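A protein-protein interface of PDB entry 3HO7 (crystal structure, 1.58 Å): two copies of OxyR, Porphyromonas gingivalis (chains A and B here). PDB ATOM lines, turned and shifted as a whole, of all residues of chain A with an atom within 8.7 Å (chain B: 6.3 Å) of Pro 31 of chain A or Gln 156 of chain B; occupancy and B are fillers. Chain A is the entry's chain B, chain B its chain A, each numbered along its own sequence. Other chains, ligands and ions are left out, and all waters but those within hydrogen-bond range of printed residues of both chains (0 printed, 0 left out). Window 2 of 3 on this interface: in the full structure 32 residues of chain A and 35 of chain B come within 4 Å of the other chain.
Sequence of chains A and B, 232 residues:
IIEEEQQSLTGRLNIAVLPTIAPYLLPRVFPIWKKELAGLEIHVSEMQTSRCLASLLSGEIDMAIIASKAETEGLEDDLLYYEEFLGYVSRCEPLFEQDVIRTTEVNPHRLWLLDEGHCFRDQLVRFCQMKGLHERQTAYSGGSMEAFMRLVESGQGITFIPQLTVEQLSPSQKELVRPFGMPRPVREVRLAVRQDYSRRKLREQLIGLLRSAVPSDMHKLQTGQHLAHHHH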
ATOM      1  N   LEU A  25     -19.319  18.094  19.877  1.00  0.00           N
ATOM      2  CA  LEU A  25     -18.923  16.817  20.457  1.00  0.00           C
ATOM      3  C   LEU A  25     -18.497  15.795  19.405  1.00  0.00           C
ATOM      4  O   LEU A  25     -17.510  15.079  19.584  1.00  0.00           O
ATOM      5  CB  LEU A  25     -20.057  16.246  21.311  1.00  0.00           C
ATOM      6  CG  LEU A  25     -19.816  14.881  21.961  1.00  0.00           C
ATOM      7  CD1 LEU A  25     -18.601  14.931  22.876  1.00  0.00           C
ATOM      8  CD2 LEU A  25     -21.054  14.433  22.721  1.00  0.00           C
ATOM      9  N   LEU A  26     -19.236  15.733  18.305  1.00  0.00           N
ATOM     10  CA  LEU A  26     -19.037  14.668  17.323  1.00  0.00           C
ATOM     11  C   LEU A  26     -17.673  14.675  16.631  1.00  0.00           C
ATOM     12  O   LEU A  26     -17.070  13.620  16.443  1.00  0.00           O
ATOM     13  CB  LEU A  26     -20.170  14.652  16.294  1.00  0.00           C
ATOM     14  CG  LEU A  26     -21.555  14.365  16.878  1.00  0.00           C
ATOM     15  CD1 LEU A  26     -22.526  13.991  15.776  1.00  0.00           C
ATOM     16  CD2 LEU A  26     -21.481  13.265  17.927  1.00  0.00           C
ATOM     17  N   PRO A  27     -17.178  15.858  16.239  1.00  0.00           N
ATOM     18  CA  PRO A  27     -15.844  15.843  15.653  1.00  0.00           C
ATOM     19  C   PRO A  27     -14.827  15.215  16.604  1.00  0.00           C
ATOM     20  O   PRO A  27     -13.825  14.659  16.156  1.00  0.00           O
ATOM     21  CB  PRO A  27     -15.545  17.327  15.439  1.00  0.00           C
ATOM     22  CG  PRO A  27     -16.887  17.941  15.236  1.00  0.00           C
ATOM     23  CD  PRO A  27     -17.818  17.182  16.137  1.00  0.00           C
ATOM     24  N   ARG A  28     -15.093  15.297  17.904  1.00  0.00           N
ATOM     25  CA  ARG A  28     -14.207  14.703  18.903  1.00  0.00           C
ATOM     26  C   ARG A  28     -14.324  13.184  18.960  1.00  0.00           C
ATOM     27  O   ARG A  28     -13.321  12.478  19.070  1.00  0.00           O
ATOM     28  CB  ARG A  28     -14.497  15.280  20.290  1.00  0.00           C
ATOM     29  CG  ARG A  28     -14.070  16.722  20.478  1.00  0.00           C
ATOM     30  CD  ARG A  28     -14.386  17.196  21.890  1.00  0.00           C
ATOM     31  NE  ARG A  28     -13.864  18.531  22.150  1.00  0.00           N
ATOM     32  CZ  ARG A  28     -12.671  18.779  22.678  1.00  0.00           C
ATOM     33  NH1 ARG A  28     -11.869  17.776  23.007  1.00  0.00           N
ATOM     34  NH2 ARG A  28     -12.279  20.028  22.880  1.00  0.00           N
ATOM     35  N   VAL A  29     -15.553  12.684  18.887  1.00  0.00           N
ATOM     36  CA  VAL A  29     -15.813  11.265  19.126  1.00  0.00           C
ATOM     37  C   VAL A  29     -15.635  10.379  17.892  1.00  0.00           C
ATOM     38  O   VAL A  29     -15.169   9.244  17.998  1.00  0.00           O
ATOM     39  CB  VAL A  29     -17.220  11.043  19.718  1.00  0.00           C
ATOM     40  CG1 VAL A  29     -17.392  11.855  20.997  1.00  0.00           C
ATOM     41  CG2 VAL A  29     -18.289  11.410  18.705  1.00  0.00           C
ATOM     42  N   PHE A  30     -16.007  10.895  16.726  1.00  0.00           N
ATOM     43  CA  PHE A  30     -15.942  10.123  15.486  1.00  0.00           C
ATOM     44  C   PHE A  30     -14.599   9.423  15.285  1.00  0.00           C
ATOM     45  O   PHE A  30     -14.554   8.254  14.898  1.00  0.00           O
ATOM     46  CB  PHE A  30     -16.268  11.018  14.288  1.00  0.00           C
ATOM     47  CG  PHE A  30     -17.740  11.260  14.095  1.00  0.00           C
ATOM     48  CD1 PHE A  30     -18.633  11.044  15.132  1.00  0.00           C
ATOM     49  CD2 PHE A  30     -18.227  11.717  12.881  1.00  0.00           C
ATOM     50  CE1 PHE A  30     -19.988  11.266  14.959  1.00  0.00           C
ATOM     51  CE2 PHE A  30     -19.580  11.946  12.703  1.00  0.00           C
ATOM     52  CZ  PHE A  30     -20.462  11.722  13.742  1.00  0.00           C
ATOM     53  N   PRO A  31     -13.495  10.140  15.538  1.00  0.00           N
ATOM     54  CA  PRO A  31     -12.164   9.546  15.424  1.00  0.00           C
ATOM     55  C   PRO A  31     -11.967   8.441  16.454  1.00  0.00           C
ATOM     56  O   PRO A  31     -11.215   7.495  16.218  1.00  0.00           O
ATOM     57  CB  PRO A  31     -11.227  10.722  15.728  1.00  0.00           C
ATOM     58  CG  PRO A  31     -12.048  11.945  15.491  1.00  0.00           C
ATOM     59  CD  PRO A  31     -13.437  11.569  15.884  1.00  0.00           C
ATOM     60  N   ILE A  32     -12.642   8.568  17.590  1.00  0.00           N
ATOM     61  CA  ILE A  32     -12.548   7.578  18.654  1.00  0.00           C
ATOM     62  C   ILE A  32     -13.360   6.334  18.306  1.00  0.00           C
ATOM     63  O   ILE A  32     -12.860   5.210  18.398  1.00  0.00           O
ATOM     64  CB  ILE A  32     -13.017   8.164  19.999  1.00  0.00           C
ATOM     65  CG1 ILE A  32     -12.077   9.295  20.429  1.00  0.00           C
ATOM     66  CG2 ILE A  32     -13.084   7.075  21.062  1.00  0.00           C
ATOM     67  CD1 ILE A  32     -12.582  10.111  21.598  1.00  0.00           C
ATOM     68  N   TRP A  33     -14.586   6.550  17.852  1.00  0.00           N
ATOM     69  CA  TRP A  33     -15.465   5.452  17.507  1.00  0.00           C
ATOM     70  C   TRP A  33     -14.860   4.617  16.395  1.00  0.00           C
ATOM     71  O   TRP A  33     -14.971   3.395  16.405  1.00  0.00           O
ATOM     72  CB  TRP A  33     -16.822   5.967  17.026  1.00  0.00           C
ATOM     73  CG  TRP A  33     -17.726   6.446  18.099  1.00  0.00           C
ATOM     74  CD1 TRP A  33     -17.569   6.283  19.441  1.00  0.00           C
ATOM     75  CD2 TRP A  33     -18.965   7.136  17.920  1.00  0.00           C
ATOM     76  NE1 TRP A  33     -18.623   6.850  20.112  1.00  0.00           N
ATOM     77  CE2 TRP A  33     -19.496   7.379  19.200  1.00  0.00           C
ATOM     78  CE3 TRP A  33     -19.673   7.583  16.801  1.00  0.00           C
ATOM     79  CZ2 TRP A  33     -20.700   8.049  19.392  1.00  0.00           C
ATOM     80  CZ3 TRP A  33     -20.866   8.245  16.994  1.00  0.00           C
ATOM     81  CH2 TRP A  33     -21.368   8.473  18.278  1.00  0.00           C
ATOM     82  N   LYS A  34     -14.239   5.266  15.420  1.00  0.00           N
ATOM     83  CA  LYS A  34     -13.740   4.499  14.300  1.00  0.00           C
ATOM     84  C   LYS A  34     -12.677   3.497  14.735  1.00  0.00           C
ATOM     85  O   LYS A  34     -12.698   2.354  14.297  1.00  0.00           O
ATOM     86  CB  LYS A  34     -13.150   5.455  13.260  1.00  0.00           C
ATOM     87  CG  LYS A  34     -12.772   4.806  11.944  1.00  0.00           C
ATOM     88  CD  LYS A  34     -14.003   4.354  11.175  1.00  0.00           C
ATOM     89  CE  LYS A  34     -13.623   3.760   9.829  1.00  0.00           C
ATOM     90  NZ  LYS A  34     -14.818   3.378   9.030  1.00  0.00           N
ATOM     91  N   LYS A  35     -11.739   3.914  15.579  1.00  0.00           N
ATOM     92  CA  LYS A  35     -10.785   2.982  16.183  1.00  0.00           C
ATOM     93  C   LYS A  35     -11.300   1.937  17.196  1.00  0.00           C
ATOM     94  O   LYS A  35     -10.883   0.782  17.175  1.00  0.00           O
ATOM     95  CB  LYS A  35      -9.525   3.700  16.681  1.00  0.00           C
ATOM     96  CG  LYS A  35      -9.442   3.922  18.167  1.00  0.00           C
ATOM     97  CD  LYS A  35      -8.017   4.277  18.556  1.00  0.00           C
ATOM     98  CE  LYS A  35      -7.575   5.581  17.912  1.00  0.00           C
ATOM     99  NZ  LYS A  35      -7.817   5.605  16.444  1.00  0.00           N
ATOM    100  N   GLU A  36     -12.198   2.370  18.084  1.00  0.00           N
ATOM    101  CA  GLU A  36     -12.675   1.551  19.207  1.00  0.00           C
ATOM    102  C   GLU A  36     -13.940   0.754  18.940  1.00  0.00           C
ATOM    103  O   GLU A  36     -14.246  -0.205  19.643  1.00  0.00           O
ATOM    104  CB  GLU A  36     -12.923   2.434  20.432  1.00  0.00           C
ATOM    105  CG  GLU A  36     -11.763   3.312  20.853  1.00  0.00           C
ATOM    106  CD  GLU A  36     -10.578   2.519  21.351  1.00  0.00           C
ATOM    107  OE1 GLU A  36      -9.496   3.114  21.523  1.00  0.00           O
ATOM    108  OE2 GLU A  36     -10.737   1.306  21.594  1.00  0.00           O
ATOM    109  N   LEU A  37     -14.678   1.178  17.931  1.00  0.00           N
ATOM    110  CA  LEU A  37     -15.943   0.563  17.551  1.00  0.00           C
ATOM    111  C   LEU A  37     -15.910   0.065  16.112  1.00  0.00           C
ATOM    112  O   LEU A  37     -16.923   0.089  15.414  1.00  0.00           O
ATOM    113  CB  LEU A  37     -17.099   1.548  17.736  1.00  0.00           C
ATOM    114  CG  LEU A  37     -17.414   1.975  19.171  1.00  0.00           C
ATOM    115  CD1 LEU A  37     -18.619   2.907  19.199  1.00  0.00           C
ATOM    116  CD2 LEU A  37     -17.653   0.758  20.052  1.00  0.00           C
ATOM    117  N   ALA A  38     -14.738  -0.380  15.672  1.00  0.00           N
ATOM    118  CA  ALA A  38     -14.598  -0.948  14.341  1.00  0.00           C
ATOM    119  C   ALA A  38     -15.500  -2.166  14.213  1.00  0.00           C
ATOM    120  O   ALA A  38     -15.491  -3.045  15.074  1.00  0.00           O
ATOM    121  CB  ALA A  38     -13.149  -1.326  14.074  1.00  0.00           C
ATOM    122  N   ALA A 213     -13.978  11.693  25.166  1.00  0.00           N
ATOM    123  CA  ALA A 213     -13.971  12.612  24.035  1.00  0.00           C
ATOM    124  C   ALA A 213     -13.814  14.055  24.502  1.00  0.00           C
ATOM    125  O   ALA A 213     -13.536  14.945  23.702  1.00  0.00           O
ATOM    126  CB  ALA A 213     -15.242  12.446  23.214  1.00  0.00           C
ATOM    127  N   SER B  90     -11.298  19.168   3.887  1.00  0.00           N
ATOM    128  CA  SER B  90     -10.376  19.049   5.010  1.00  0.00           C
ATOM    129  C   SER B  90      -8.944  18.931   4.502  1.00  0.00           C
ATOM    130  O   SER B  90      -8.709  18.473   3.385  1.00  0.00           O
ATOM    131  CB  SER B  90     -10.716  17.838   5.876  1.00  0.00           C
ATOM    132  OG  SER B  90      -9.818  16.773   5.621  1.00  0.00           O
ATOM    133  N   CYS B  92      -6.878  16.903   5.200  1.00  0.00           N
ATOM    134  CA  CYS B  92      -6.479  15.498   5.142  1.00  0.00           C
ATOM    135  C   CYS B  92      -6.933  14.811   3.857  1.00  0.00           C
ATOM    136  O   CYS B  92      -6.498  13.702   3.551  1.00  0.00           O
ATOM    137  CB  CYS B  92      -7.024  14.737   6.351  1.00  0.00           C
ATOM    138  SG  CYS B  92      -6.646  15.507   7.937  1.00  0.00           S
ATOM    139  N   GLU B  93      -7.813  15.466   3.107  1.00  0.00           N
ATOM    140  CA  GLU B  93      -8.328  14.883   1.873  1.00  0.00           C
ATOM    141  C   GLU B  93      -7.343  15.061   0.723  1.00  0.00           C
ATOM    142  O   GLU B  93      -6.762  16.133   0.559  1.00  0.00           O
ATOM    143  CB  GLU B  93      -9.675  15.508   1.502  1.00  0.00           C
ATOM    144  CG  GLU B  93     -10.588  15.767   2.690  1.00  0.00           C
ATOM    145  CD  GLU B  93     -10.829  14.527   3.528  1.00  0.00           C
ATOM    146  OE1 GLU B  93     -11.156  13.465   2.952  1.00  0.00           O
ATOM    147  OE2 GLU B  93     -10.692  14.614   4.768  1.00  0.00           O
ATOM    148  N   ARG B 110     -16.359   9.796   2.661  1.00  0.00           N
ATOM    149  CA  ARG B 110     -15.889  10.912   3.477  1.00  0.00           C
ATOM    150  C   ARG B 110     -16.615  12.205   3.122  1.00  0.00           C
ATOM    151  O   ARG B 110     -16.066  13.296   3.267  1.00  0.00           O
ATOM    152  CB  ARG B 110     -14.376  11.089   3.326  1.00  0.00           C
ATOM    153  CG  ARG B 110     -13.569   9.880   3.778  1.00  0.00           C
ATOM    154  CD  ARG B 110     -12.081  10.072   3.533  1.00  0.00           C
ATOM    155  NE  ARG B 110     -11.534  11.183   4.305  1.00  0.00           N
ATOM    156  CZ  ARG B 110     -11.274  11.132   5.608  1.00  0.00           C
ATOM    157  NH1 ARG B 110     -11.518  10.021   6.292  1.00  0.00           N
ATOM    158  NH2 ARG B 110     -10.773  12.191   6.229  1.00  0.00           N
ATOM    159  N   TRP B 112     -20.040  14.665   3.633  1.00  0.00           N
ATOM    160  CA  TRP B 112     -21.152  14.984   4.515  1.00  0.00           C
ATOM    161  C   TRP B 112     -22.172  15.773   3.716  1.00  0.00           C
ATOM    162  O   TRP B 112     -21.882  16.859   3.227  1.00  0.00           O
ATOM    163  CB  TRP B 112     -20.675  15.809   5.710  1.00  0.00           C
ATOM    164  CG  TRP B 112     -19.536  15.188   6.452  1.00  0.00           C
ATOM    165  CD1 TRP B 112     -18.242  15.610   6.467  1.00  0.00           C
ATOM    166  CD2 TRP B 112     -19.589  14.024   7.282  1.00  0.00           C
ATOM    167  NE1 TRP B 112     -17.483  14.785   7.258  1.00  0.00           N
ATOM    168  CE2 TRP B 112     -18.287  13.802   7.770  1.00  0.00           C
ATOM    169  CE3 TRP B 112     -20.609  13.148   7.661  1.00  0.00           C
ATOM    170  CZ2 TRP B 112     -17.980  12.742   8.618  1.00  0.00           C
ATOM    171  CZ3 TRP B 112     -20.303  12.098   8.500  1.00  0.00           C
ATOM    172  CH2 TRP B 112     -18.999  11.904   8.971  1.00  0.00           C
ATOM    173  N   PHE B 148     -21.127  19.808  10.130  1.00  0.00           N
ATOM    174  CA  PHE B 148     -20.334  19.391   8.973  1.00  0.00           C
ATOM    175  C   PHE B 148     -19.059  20.221   8.814  1.00  0.00           C
ATOM    176  O   PHE B 148     -17.988  19.679   8.561  1.00  0.00           O
ATOM    177  CB  PHE B 148     -21.151  19.454   7.682  1.00  0.00           C
ATOM    178  CG  PHE B 148     -22.269  18.456   7.616  1.00  0.00           C
ATOM    179  CD1 PHE B 148     -22.262  17.329   8.421  1.00  0.00           C
ATOM    180  CD2 PHE B 148     -23.317  18.633   6.727  1.00  0.00           C
ATOM    181  CE1 PHE B 148     -23.294  16.406   8.355  1.00  0.00           C
ATOM    182  CE2 PHE B 148     -24.350  17.716   6.655  1.00  0.00           C
ATOM    183  CZ  PHE B 148     -24.337  16.599   7.468  1.00  0.00           C
ATOM    184  N   ARG B 150     -17.491  21.878  11.143  1.00  0.00           N
ATOM    185  CA  ARG B 150     -16.624  21.573  12.268  1.00  0.00           C
ATOM    186  C   ARG B 150     -15.865  20.277  11.988  1.00  0.00           C
ATOM    187  O   ARG B 150     -14.694  20.146  12.339  1.00  0.00           O
ATOM    188  CB  ARG B 150     -17.429  21.464  13.564  1.00  0.00           C
ATOM    189  CG  ARG B 150     -18.146  22.746  13.977  1.00  0.00           C
ATOM    190  CD  ARG B 150     -17.169  23.881  14.233  1.00  0.00           C
ATOM    191  NE  ARG B 150     -16.897  24.638  13.017  1.00  0.00           N
ATOM    192  CZ  ARG B 150     -17.704  25.576  12.528  1.00  0.00           C
ATOM    193  NH1 ARG B 150     -17.384  26.217  11.412  1.00  0.00           N
ATOM    194  NH2 ARG B 150     -18.833  25.872  13.156  1.00  0.00           N
ATOM    195  N   LEU B 151     -16.532  19.329  11.339  1.00  0.00           N
ATOM    196  CA  LEU B 151     -15.896  18.051  11.018  1.00  0.00           C
ATOM    197  C   LEU B 151     -14.767  18.260  10.020  1.00  0.00           C
ATOM    198  O   LEU B 151     -13.648  17.782  10.215  1.00  0.00           O
ATOM    199  CB  LEU B 151     -16.919  17.058  10.463  1.00  0.00           C
ATOM    200  CG  LEU B 151     -17.875  16.440  11.484  1.00  0.00           C
ATOM    201  CD1 LEU B 151     -19.019  15.715  10.785  1.00  0.00           C
ATOM    202  CD2 LEU B 151     -17.118  15.508  12.409  1.00  0.00           C
ATOM    203  N   VAL B 152     -15.064  18.988   8.950  1.00  0.00           N
ATOM    204  CA  VAL B 152     -14.076  19.255   7.914  1.00  0.00           C
ATOM    205  C   VAL B 152     -12.861  19.986   8.478  1.00  0.00           C
ATOM    206  O   VAL B 152     -11.721  19.637   8.175  1.00  0.00           O
ATOM    207  CB  VAL B 152     -14.682  20.067   6.753  1.00  0.00           C
ATOM    208  CG1 VAL B 152     -13.608  20.430   5.740  1.00  0.00           C
ATOM    209  CG2 VAL B 152     -15.806  19.282   6.095  1.00  0.00           C
ATOM    210  N   GLU B 153     -13.108  20.994   9.306  1.00  0.00           N
ATOM    211  CA  GLU B 153     -12.027  21.777   9.893  1.00  0.00           C
ATOM    212  C   GLU B 153     -11.131  20.933  10.799  1.00  0.00           C
ATOM    213  O   GLU B 153      -9.988  21.295  11.071  1.00  0.00           O
ATOM    214  CB  GLU B 153     -12.597  22.979  10.647  1.00  0.00           C
ATOM    215  CG  GLU B 153     -13.367  23.938   9.749  1.00  0.00           C
ATOM    216  CD  GLU B 153     -14.256  24.884  10.528  1.00  0.00           C
ATOM    217  OE1 GLU B 153     -14.225  24.839  11.778  1.00  0.00           O
ATOM    218  OE2 GLU B 153     -14.993  25.665   9.888  1.00  0.00           O
ATOM    219  N   SER B 154     -11.679  19.812  11.259  1.00  0.00           N
ATOM    220  CA  SER B 154     -10.984  18.894  12.150  1.00  0.00           C
ATOM    221  C   SER B 154     -10.243  17.827  11.355  1.00  0.00           C
ATOM    222  O   SER B 154      -9.637  16.924  11.926  1.00  0.00           O
ATOM    223  CB  SER B 154     -11.963  18.245  13.129  1.00  0.00           C
ATOM    224  OG  SER B 154     -12.988  17.556  12.442  1.00  0.00           O
ATOM    225  N   GLY B 155     -10.296  17.941  10.034  1.00  0.00           N
ATOM    226  CA  GLY B 155      -9.632  16.993   9.161  1.00  0.00           C
ATOM    227  C   GLY B 155     -10.446  15.783   8.748  1.00  0.00           C
ATOM    228  O   GLY B 155      -9.914  14.860   8.138  1.00  0.00           O
ATOM    229  N   GLN B 156     -11.732  15.765   9.075  1.00  0.00           N
ATOM    230  CA  GLN B 156     -12.544  14.639   8.656  1.00  0.00           C
ATOM    231  C   GLN B 156     -13.499  15.008   7.529  1.00  0.00           C
ATOM    232  O   GLN B 156     -14.478  15.718   7.732  1.00  0.00           O
ATOM    233  CB  GLN B 156     -13.346  14.118   9.851  1.00  0.00           C
ATOM    234  CG  GLN B 156     -12.545  14.029  11.142  1.00  0.00           C
ATOM    235  CD  GLN B 156     -13.408  13.709  12.350  1.00  0.00           C
ATOM    236  OE1 GLN B 156     -14.379  12.963  12.254  1.00  0.00           O
ATOM    237  NE2 GLN B 156     -13.052  14.274  13.496  1.00  0.00           N
ATOM    238  N   GLY B 157     -13.245  14.448   6.354  1.00  0.00           N
ATOM    239  CA  GLY B 157     -14.128  14.599   5.218  1.00  0.00           C
ATOM    240  C   GLY B 157     -14.227  15.908   4.458  1.00  0.00           C
ATOM    241  O   GLY B 157     -13.387  16.802   4.539  1.00  0.00           O
ATOM    242  N   ILE B 158     -15.313  15.979   3.703  1.00  0.00           N
ATOM    243  CA  ILE B 158     -15.681  17.084   2.843  1.00  0.00           C
ATOM    244  C   ILE B 158     -17.169  17.381   2.948  1.00  0.00           C
ATOM    245  O   ILE B 158     -17.974  16.496   3.239  1.00  0.00           O
ATOM    246  CB  ILE B 158     -15.359  16.748   1.373  1.00  0.00           C
ATOM    247  CG1 ILE B 158     -13.844  16.714   1.149  1.00  0.00           C
ATOM    248  CG2 ILE B 158     -16.055  17.722   0.436  1.00  0.00           C
ATOM    249  CD1 ILE B 158     -13.440  16.450  -0.289  1.00  0.00           C
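The side-chain amide nitrogen of Gln 156 of chain B sits at hydrogen-bond distance from the backbone carbonyl oxygen of Pro 27 of chain A, 2.8 Å away.
Of the printed residues of chain B, Pro 31 of chain A touches Gln 156 (3.2 Å).
Gln 156 of chain B touches three residues of chain A.
Printed residues of chain B within 4 Å of Phe 30 of chain A: Trp 112 (3.8 Å), Leu 151 (3.98 Å) and Gln 156 (3.4 Å).
Printed residues of chain A within 4 Å of Leu 151 of chain B: Pro 27 (3.5 Å) and Phe 30 (3.98 Å).
Of the printed residues of chain A, Arg 150 of chain B touches Pro 27.
Printed residues of chain A within 4 Å of Trp 112 of chain B: Phe 30 (3.8 Å).
Leu 26 of chain A touches none of the printed residues of chain B.
The nearest printed residue of chain B that does not touch Pro 31 of chain A is Leu 151 of chain B (6.4 Å).
The nearest residue of chain A that does not touch Gln 156 of chain B is Arg 28 of chain A (5.0 Å).
No position is printed for both chains.
Arg 150 of chain B touches Pro 27 of chain A (CB to CG, 3.9 Å).
Pro 27 of chain A touches Leu 151 of chain B.
Pro 27 of chain A touches Ser 154 of chain B.
Trp 112 of chain B touches Phe 30 of chain A (CH2 to CE2, 3.8 Å).
Leu 151 of chain B touches Phe 30 of chain A.
OE1 of Gln 156 of chain B touches CB of Phe 30 of chain A (3.4 Å).
NE2 of Gln 156 of chain B touches CG of Pro 31 of chain A (3.2 Å).
The indole nitrogen (NE1) of Trp 112 of chain B is in hydrogen-bond range of the backbone carbonyl oxygen (O) of Gln 156 of chain B, at 3.2 Å.
The guanidinium group (NH1) of Arg 150 of chain B lies within salt-bridge range of the side-chain carboxylate (OE2) of Glu 153 of chain B (2.9 Å).
O of Arg 150 of chain B lies within hydrogen-bond range of OG of Ser 154 of chain B (3.1 Å).
The side-chain hydroxyl (OG) of Ser 154 of chain B lies within hydrogen-bond range of the side-chain amide nitrogen (NE2) of Gln 156 of chain B (3.4 Å).
O of Ile 158 of chain B lies within hydrogen-bond range of N of Trp 112 of chain B (2.8 Å).
The backbone carbonyl oxygen (O) of Leu 151 of chain B is in hydrogen-bond range of the backbone NH (N) of Gln 156 of chain B, at 3.0 Å.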
